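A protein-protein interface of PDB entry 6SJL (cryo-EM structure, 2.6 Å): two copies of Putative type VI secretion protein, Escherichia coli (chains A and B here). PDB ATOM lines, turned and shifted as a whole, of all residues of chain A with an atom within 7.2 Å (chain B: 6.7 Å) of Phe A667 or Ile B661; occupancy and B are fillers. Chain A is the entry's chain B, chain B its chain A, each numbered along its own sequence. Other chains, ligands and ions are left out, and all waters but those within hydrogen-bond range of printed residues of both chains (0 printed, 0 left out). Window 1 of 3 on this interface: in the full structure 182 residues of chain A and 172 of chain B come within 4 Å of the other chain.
Phe A667 touches two residues of chain B.
Ile B661 touches four residues of chain A.
Printed residues of chain B within 4 Å of Gly A664: Asp B657 (3.5 Å).
Of the printed residues of chain A, Thr B659 touches Ile A661 (3.7 Å), Ala A663 (3.99 Å), Ser A666 (3.0 Å), Phe A667 (3.3 Å) and Thr A668 (3.1 Å).
Printed residues of chain A within 4 Å of Ala B663: Val A670 and Ala A671.
Printed residues of chain A within 4 Å of Asp B660: Thr A668 (2.9 Å).
Printed residues of chain B within 4 Å of Val A670: Ile B661, Thr B662 and Ala B663.
The nearest residue of chain B that does not touch Phe A667 is Leu B677 (4.5 Å).
The nearest residue of chain A that does not touch Ile B661 is Ile A661 (4.3 Å).
The nearest printed residue of chain A that does not touch Asp B660 is Ser A666 (5.2 Å).
Thr B659 touches Ile A661.
Ala A663 touches Thr B659 (CB to OG1, 3.99 Å).
Asn B658 touches Gln A665 (OD1 to CB, 3.0 Å).
Phe A667 touches Thr B659.
O of Ile B661 touches CA of Val A669 (3.3 Å).
O of Ala B663 touches CA of Ala A671, 3.5 Å away.
Ala A671 touches Ser B666 (CB to C, 3.9 Å).
N of Phe B667 touches CB of Ala A671, 3.7 Å away.
CD2 of Leu A677 touches CE2 of Phe B667 (3.8 Å).
Leu A677 touches Leu B677 (CD1 to CD1, 3.8 Å).
O of Ser A666 is in hydrogen-bond range of N of Thr B659 (3.0 Å).
The backbone carbonyl oxygen of Ile B653 lies within hydrogen-bond range of the backbone NH of Thr A662, 2.8 Å away.
O of Asp B657 is in hydrogen-bond range of N of Gly A664, 3.5 Å away.
O of Thr B659 lies within hydrogen-bond range of N of Thr A668, at 3.1 Å.
O of Asp B657 sits at hydrogen-bond distance from N of Gln A665, at 3.3 Å.
The backbone carbonyl oxygen (O) of Thr A668 is in hydrogen-bond range of the backbone NH (N) of Ile B661, 2.9 Å away.
The backbone NH of Val A670 lies within hydrogen-bond range of the backbone carbonyl oxygen of Ile B661 (3.0 Å).
The backbone NH (N) of Ala B663 sits at hydrogen-bond distance from the backbone carbonyl oxygen (O) of Val A670, at 3.0 Å.
The side-chain amide oxygen (OD1) of Asn B658 sits at hydrogen-bond distance from the backbone NH (N) of Ser A666, 3.1 Å away.
The side-chain carboxylate (OD1) of Asp B660 is in hydrogen-bond range of the side-chain hydroxyl (OG1) of Thr A668, at 2.9 Å.
The side-chain amide nitrogen (ND2) of Asn B658 lies close to the side-chain carboxylate (OD1) of Asp B660 (3.3 Å).
Printed residues of chain B that touch a printed residue of chain A: Ile B653, Asp B657, Asn B658, Thr B659, Asp B660, Ile B661, Thr B662, Ala B663, Ser B666, Phe B667 and Leu B677.
Among the printed residues, 25 pairs touch across the chains.
Ile A661 touches Ile B653, but with the chains exchanged Ile A653 does not touch Ile B661 (5.8 Å).
Phe A667 touches Ile B661, but with the chains exchanged Ile A661 does not touch Phe B667 (6.2 Å).
Leu A677 touches Phe B667, but with the chains exchanged Phe A667 does not touch Leu B677 (4.5 Å).
Leu B677 touches its own counterpart, Leu A677.
Positions printed for both chains: 653, 661, 662, 663, 666, 667 and 677.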
ATOM      1  N   ILE A 653     -35.928  -0.745 -21.702  1.00  0.00           N
ATOM      2  CA  ILE A 653     -36.809   0.355 -21.367  1.00  0.00           C
ATOM      3  C   ILE A 653     -38.036   0.210 -22.236  1.00  0.00           C
ATOM      4  O   ILE A 653     -38.011   0.534 -23.423  1.00  0.00           O
ATOM      5  CB  ILE A 653     -36.140   1.710 -21.573  1.00  0.00           C
ATOM      6  CG1 ILE A 653     -34.933   1.816 -20.662  1.00  0.00           C
ATOM      7  CG2 ILE A 653     -37.104   2.793 -21.273  1.00  0.00           C
ATOM      8  CD1 ILE A 653     -33.950   2.799 -21.123  1.00  0.00           C
ATOM      9  N   ILE A 661     -36.131  10.976 -23.897  1.00  0.00           N
ATOM     10  CA  ILE A 661     -34.859  11.309 -23.288  1.00  0.00           C
ATOM     11  C   ILE A 661     -34.645  12.790 -23.495  1.00  0.00           C
ATOM     12  O   ILE A 661     -34.769  13.292 -24.611  1.00  0.00           O
ATOM     13  CB  ILE A 661     -33.714  10.486 -23.876  1.00  0.00           C
ATOM     14  CG1 ILE A 661     -33.952   9.019 -23.586  1.00  0.00           C
ATOM     15  CG2 ILE A 661     -32.428  10.921 -23.289  1.00  0.00           C
ATOM     16  CD1 ILE A 661     -32.901   8.148 -24.103  1.00  0.00           C
ATOM     17  N   THR A 662     -34.380  13.497 -22.415  1.00  0.00           N
ATOM     18  CA  THR A 662     -34.151  14.931 -22.438  1.00  0.00           C
ATOM     19  C   THR A 662     -32.814  15.182 -21.773  1.00  0.00           C
ATOM     20  O   THR A 662     -32.689  15.025 -20.562  1.00  0.00           O
ATOM     21  CB  THR A 662     -35.269  15.672 -21.719  1.00  0.00           C
ATOM     22  OG1 THR A 662     -36.470  15.589 -22.481  1.00  0.00           O
ATOM     23  CG2 THR A 662     -34.917  17.074 -21.564  1.00  0.00           C
ATOM     24  N   ALA A 663     -31.819  15.567 -22.549  1.00  0.00           N
ATOM     25  CA  ALA A 663     -30.480  15.788 -22.038  1.00  0.00           C
ATOM     26  C   ALA A 663     -30.202  17.277 -22.048  1.00  0.00           C
ATOM     27  O   ALA A 663     -30.476  17.954 -23.035  1.00  0.00           O
ATOM     28  CB  ALA A 663     -29.451  15.026 -22.857  1.00  0.00           C
ATOM     29  N   GLY A 664     -29.737  17.795 -20.917  1.00  0.00           N
ATOM     30  CA  GLY A 664     -29.326  19.181 -20.864  1.00  0.00           C
ATOM     31  C   GLY A 664     -28.021  19.425 -21.579  1.00  0.00           C
ATOM     32  O   GLY A 664     -27.750  20.542 -22.009  1.00  0.00           O
ATOM     33  N   GLN A 665     -27.153  18.440 -21.595  1.00  0.00           N
ATOM     34  CA  GLN A 665     -26.009  18.287 -22.475  1.00  0.00           C
ATOM     35  C   GLN A 665     -26.322  17.283 -23.588  1.00  0.00           C
ATOM     36  O   GLN A 665     -27.446  17.199 -24.064  1.00  0.00           O
ATOM     37  CB  GLN A 665     -24.779  17.920 -21.662  1.00  0.00           C
ATOM     38  CG  GLN A 665     -24.253  19.039 -20.809  1.00  0.00           C
ATOM     39  CD  GLN A 665     -24.162  20.359 -21.525  1.00  0.00           C
ATOM     40  OE1 GLN A 665     -23.835  20.425 -22.706  1.00  0.00           O
ATOM     41  NE2 GLN A 665     -24.414  21.429 -20.799  1.00  0.00           N
ATOM     42  N   SER A 666     -25.295  16.621 -24.096  1.00  0.00           N
ATOM     43  CA  SER A 666     -25.408  15.672 -25.191  1.00  0.00           C
ATOM     44  C   SER A 666     -26.189  14.419 -24.808  1.00  0.00           C
ATOM     45  O   SER A 666     -26.346  14.083 -23.649  1.00  0.00           O
ATOM     46  CB  SER A 666     -24.022  15.257 -25.646  1.00  0.00           C
ATOM     47  OG  SER A 666     -23.345  16.337 -26.245  1.00  0.00           O
ATOM     48  N   PHE A 667     -26.677  13.716 -25.820  1.00  0.00           N
ATOM     49  CA  PHE A 667     -27.198  12.362 -25.682  1.00  0.00           C
ATOM     50  C   PHE A 667     -26.357  11.464 -26.563  1.00  0.00           C
ATOM     51  O   PHE A 667     -26.369  11.606 -27.782  1.00  0.00           O
ATOM     52  CB  PHE A 667     -28.657  12.271 -26.100  1.00  0.00           C
ATOM     53  CG  PHE A 667     -29.115  10.877 -26.391  1.00  0.00           C
ATOM     54  CD1 PHE A 667     -29.354   9.989 -25.380  1.00  0.00           C
ATOM     55  CD2 PHE A 667     -29.314  10.457 -27.681  1.00  0.00           C
ATOM     56  CE1 PHE A 667     -29.771   8.734 -25.648  1.00  0.00           C
ATOM     57  CE2 PHE A 667     -29.736   9.193 -27.939  1.00  0.00           C
ATOM     58  CZ  PHE A 667     -29.966   8.339 -26.921  1.00  0.00           C
ATOM     59  N   THR A 668     -25.618  10.558 -25.957  1.00  0.00           N
ATOM     60  CA  THR A 668     -24.662   9.759 -26.689  1.00  0.00           C
ATOM     61  C   THR A 668     -24.990   8.292 -26.513  1.00  0.00           C
ATOM     62  O   THR A 668     -25.436   7.874 -25.453  1.00  0.00           O
ATOM     63  CB  THR A 668     -23.242  10.047 -26.219  1.00  0.00           C
ATOM     64  OG1 THR A 668     -23.061   9.522 -24.906  1.00  0.00           O
ATOM     65  CG2 THR A 668     -23.004  11.529 -26.161  1.00  0.00           C
ATOM     66  N   VAL A 669     -24.813   7.521 -27.570  1.00  0.00           N
ATOM     67  CA  VAL A 669     -24.907   6.074 -27.521  1.00  0.00           C
ATOM     68  C   VAL A 669     -23.627   5.523 -28.110  1.00  0.00           C
ATOM     69  O   VAL A 669     -23.147   6.029 -29.124  1.00  0.00           O
ATOM     70  CB  VAL A 669     -26.132   5.541 -28.283  1.00  0.00           C
ATOM     71  CG1 VAL A 669     -26.156   4.064 -28.249  1.00  0.00           C
ATOM     72  CG2 VAL A 669     -27.376   6.068 -27.693  1.00  0.00           C
ATOM     73  N   VAL A 670     -23.032   4.548 -27.443  1.00  0.00           N
ATOM     74  CA  VAL A 670     -21.961   3.762 -28.021  1.00  0.00           C
ATOM     75  C   VAL A 670     -22.348   2.312 -27.833  1.00  0.00           C
ATOM     76  O   VAL A 670     -22.432   1.833 -26.702  1.00  0.00           O
ATOM     77  CB  VAL A 670     -20.592   4.043 -27.384  1.00  0.00           C
ATOM     78  CG1 VAL A 670     -19.521   3.325 -28.148  1.00  0.00           C
ATOM     79  CG2 VAL A 670     -20.297   5.489 -27.369  1.00  0.00           C
ATOM     80  N   ALA A 671     -22.588   1.615 -28.929  1.00  0.00           N
ATOM     81  CA  ALA A 671     -22.929   0.208 -28.901  1.00  0.00           C
ATOM     82  C   ALA A 671     -21.792  -0.557 -29.536  1.00  0.00           C
ATOM     83  O   ALA A 671     -21.321  -0.184 -30.606  1.00  0.00           O
ATOM     84  CB  ALA A 671     -24.225  -0.067 -29.641  1.00  0.00           C
ATOM     85  N   LEU A 677     -32.480   2.096 -34.903  1.00  0.00           N
ATOM     86  CA  LEU A 677     -33.670   2.831 -34.529  1.00  0.00           C
ATOM     87  C   LEU A 677     -34.717   2.509 -35.568  1.00  0.00           C
ATOM     88  O   LEU A 677     -34.591   2.919 -36.716  1.00  0.00           O
ATOM     89  CB  LEU A 677     -33.397   4.325 -34.478  1.00  0.00           C
ATOM     90  CG  LEU A 677     -32.138   4.788 -33.778  1.00  0.00           C
ATOM     91  CD1 LEU A 677     -31.972   6.238 -34.028  1.00  0.00           C
ATOM     92  CD2 LEU A 677     -32.308   4.564 -32.338  1.00  0.00           C
ATOM     93  N   ILE B 653     -36.489   9.985 -19.306  1.00  0.00           N
ATOM     94  CA  ILE B 653     -35.137  10.085 -18.792  1.00  0.00           C
ATOM     95  C   ILE B 653     -34.709  11.522 -18.983  1.00  0.00           C
ATOM     96  O   ILE B 653     -34.516  11.974 -20.111  1.00  0.00           O
ATOM     97  CB  ILE B 653     -34.175   9.123 -19.486  1.00  0.00           C
ATOM     98  CG1 ILE B 653     -34.545   7.694 -19.156  1.00  0.00           C
ATOM     99  CG2 ILE B 653     -32.793   9.378 -19.021  1.00  0.00           C
ATOM    100  CD1 ILE B 653     -34.250   6.750 -20.238  1.00  0.00           C
ATOM    101  N   ASP B 657     -26.768  16.943 -17.345  1.00  0.00           N
ATOM    102  CA  ASP B 657     -25.660  16.689 -18.250  1.00  0.00           C
ATOM    103  C   ASP B 657     -26.092  15.704 -19.335  1.00  0.00           C
ATOM    104  O   ASP B 657     -27.240  15.690 -19.771  1.00  0.00           O
ATOM    105  CB  ASP B 657     -24.450  16.179 -17.482  1.00  0.00           C
ATOM    106  CG  ASP B 657     -23.730  17.265 -16.747  1.00  0.00           C
ATOM    107  OD1 ASP B 657     -22.830  16.932 -15.949  1.00  0.00           O
ATOM    108  OD2 ASP B 657     -24.070  18.446 -16.946  1.00  0.00           O
ATOM    109  N   ASN B 658     -25.134  14.963 -19.867  1.00  0.00           N
ATOM    110  CA  ASN B 658     -25.374  13.910 -20.840  1.00  0.00           C
ATOM    111  C   ASN B 658     -26.363  12.845 -20.400  1.00  0.00           C
ATOM    112  O   ASN B 658     -26.546  12.600 -19.214  1.00  0.00           O
ATOM    113  CB  ASN B 658     -24.065  13.216 -21.180  1.00  0.00           C
ATOM    114  CG  ASN B 658     -23.133  14.091 -21.931  1.00  0.00           C
ATOM    115  OD1 ASN B 658     -23.371  15.267 -22.095  1.00  0.00           O
ATOM    116  ND2 ASN B 658     -22.074  13.511 -22.434  1.00  0.00           N
ATOM    117  N   THR B 659     -26.999  12.193 -21.359  1.00  0.00           N
ATOM    118  CA  THR B 659     -27.610  10.891 -21.149  1.00  0.00           C
ATOM    119  C   THR B 659     -26.810   9.942 -22.013  1.00  0.00           C
ATOM    120  O   THR B 659     -26.894  10.000 -23.237  1.00  0.00           O
ATOM    121  CB  THR B 659     -29.079  10.850 -21.534  1.00  0.00           C
ATOM    122  OG1 THR B 659     -29.829  11.709 -20.681  1.00  0.00           O
ATOM    123  CG2 THR B 659     -29.596   9.450 -21.365  1.00  0.00           C
ATOM    124  N   ASP B 660     -26.016   9.098 -21.388  1.00  0.00           N
ATOM    125  CA  ASP B 660     -25.126   8.202 -22.093  1.00  0.00           C
ATOM    126  C   ASP B 660     -25.710   6.811 -22.031  1.00  0.00           C
ATOM    127  O   ASP B 660     -26.063   6.340 -20.956  1.00  0.00           O
ATOM    128  CB  ASP B 660     -23.742   8.216 -21.473  1.00  0.00           C
ATOM    129  CG  ASP B 660     -23.259   9.604 -21.176  1.00  0.00           C
ATOM    130  OD1 ASP B 660     -23.032  10.361 -22.134  1.00  0.00           O
ATOM    131  OD2 ASP B 660     -23.128   9.947 -19.978  1.00  0.00           O
ATOM    132  N   ILE B 661     -25.829   6.161 -23.174  1.00  0.00           N
ATOM    133  CA  ILE B 661     -26.136   4.747 -23.229  1.00  0.00           C
ATOM    134  C   ILE B 661     -24.904   4.035 -23.741  1.00  0.00           C
ATOM    135  O   ILE B 661     -24.266   4.495 -24.687  1.00  0.00           O
ATOM    136  CB  ILE B 661     -27.365   4.464 -24.096  1.00  0.00           C
ATOM    137  CG1 ILE B 661     -28.599   5.002 -23.401  1.00  0.00           C
ATOM    138  CG2 ILE B 661     -27.496   3.010 -24.324  1.00  0.00           C
ATOM    139  CD1 ILE B 661     -29.722   5.218 -24.295  1.00  0.00           C
ATOM    140  N   THR B 662     -24.527   2.962 -23.069  1.00  0.00           N
ATOM    141  CA  THR B 662     -23.343   2.192 -23.409  1.00  0.00           C
ATOM    142  C   THR B 662     -23.767   0.740 -23.453  1.00  0.00           C
ATOM    143  O   THR B 662     -24.138   0.172 -22.433  1.00  0.00           O
ATOM    144  CB  THR B 662     -22.238   2.406 -22.384  1.00  0.00           C
ATOM    145  OG1 THR B 662     -21.742   3.736 -22.481  1.00  0.00           O
ATOM    146  CG2 THR B 662     -21.130   1.480 -22.626  1.00  0.00           C
ATOM    147  N   ALA B 663     -23.739   0.140 -24.625  1.00  0.00           N
ATOM    148  CA  ALA B 663     -24.172  -1.230 -24.793  1.00  0.00           C
ATOM    149  C   ALA B 663     -22.985  -2.078 -25.201  1.00  0.00           C
ATOM    150  O   ALA B 663     -22.212  -1.683 -26.066  1.00  0.00           O
ATOM    151  CB  ALA B 663     -25.283  -1.312 -25.819  1.00  0.00           C
ATOM    152  N   SER B 666     -25.737  -4.566 -29.060  1.00  0.00           N
ATOM    153  CA  SER B 666     -26.436  -3.530 -29.803  1.00  0.00           C
ATOM    154  C   SER B 666     -27.177  -2.546 -28.901  1.00  0.00           C
ATOM    155  O   SER B 666     -27.333  -2.738 -27.712  1.00  0.00           O
ATOM    156  CB  SER B 666     -27.435  -4.163 -30.756  1.00  0.00           C
ATOM    157  OG  SER B 666     -26.795  -5.071 -31.617  1.00  0.00           O
ATOM    158  N   PHE B 667     -27.626  -1.458 -29.512  1.00  0.00           N
ATOM    159  CA  PHE B 667     -28.582  -0.524 -28.938  1.00  0.00           C
ATOM    160  C   PHE B 667     -29.766  -0.472 -29.878  1.00  0.00           C
ATOM    161  O   PHE B 667     -29.613  -0.123 -31.045  1.00  0.00           O
ATOM    162  CB  PHE B 667     -27.992   0.869 -28.778  1.00  0.00           C
ATOM    163  CG  PHE B 667     -29.013   1.928 -28.509  1.00  0.00           C
ATOM    164  CD1 PHE B 667     -29.578   2.063 -27.270  1.00  0.00           C
ATOM    165  CD2 PHE B 667     -29.407   2.787 -29.500  1.00  0.00           C
ATOM    166  CE1 PHE B 667     -30.498   3.018 -27.032  1.00  0.00           C
ATOM    167  CE2 PHE B 667     -30.332   3.742 -29.253  1.00  0.00           C
ATOM    168  CZ  PHE B 667     -30.875   3.855 -28.021  1.00  0.00           C
ATOM    169  N   LEU B 677     -34.838  12.270 -32.978  1.00  0.00           N
ATOM    170  CA  LEU B 677     -33.656  12.739 -32.278  1.00  0.00           C
ATOM    171  C   LEU B 677     -33.435  14.191 -32.639  1.00  0.00           C
ATOM    172  O   LEU B 677     -33.278  14.519 -33.810  1.00  0.00           O
ATOM    173  CB  LEU B 677     -32.432  11.917 -32.647  1.00  0.00           C
ATOM    174  CG  LEU B 677     -32.555  10.411 -32.657  1.00  0.00           C
ATOM    175  CD1 LEU B 677     -31.294   9.868 -33.215  1.00  0.00           C
ATOM    176  CD2 LEU B 677     -32.732   9.941 -31.275  1.00  0.00           C
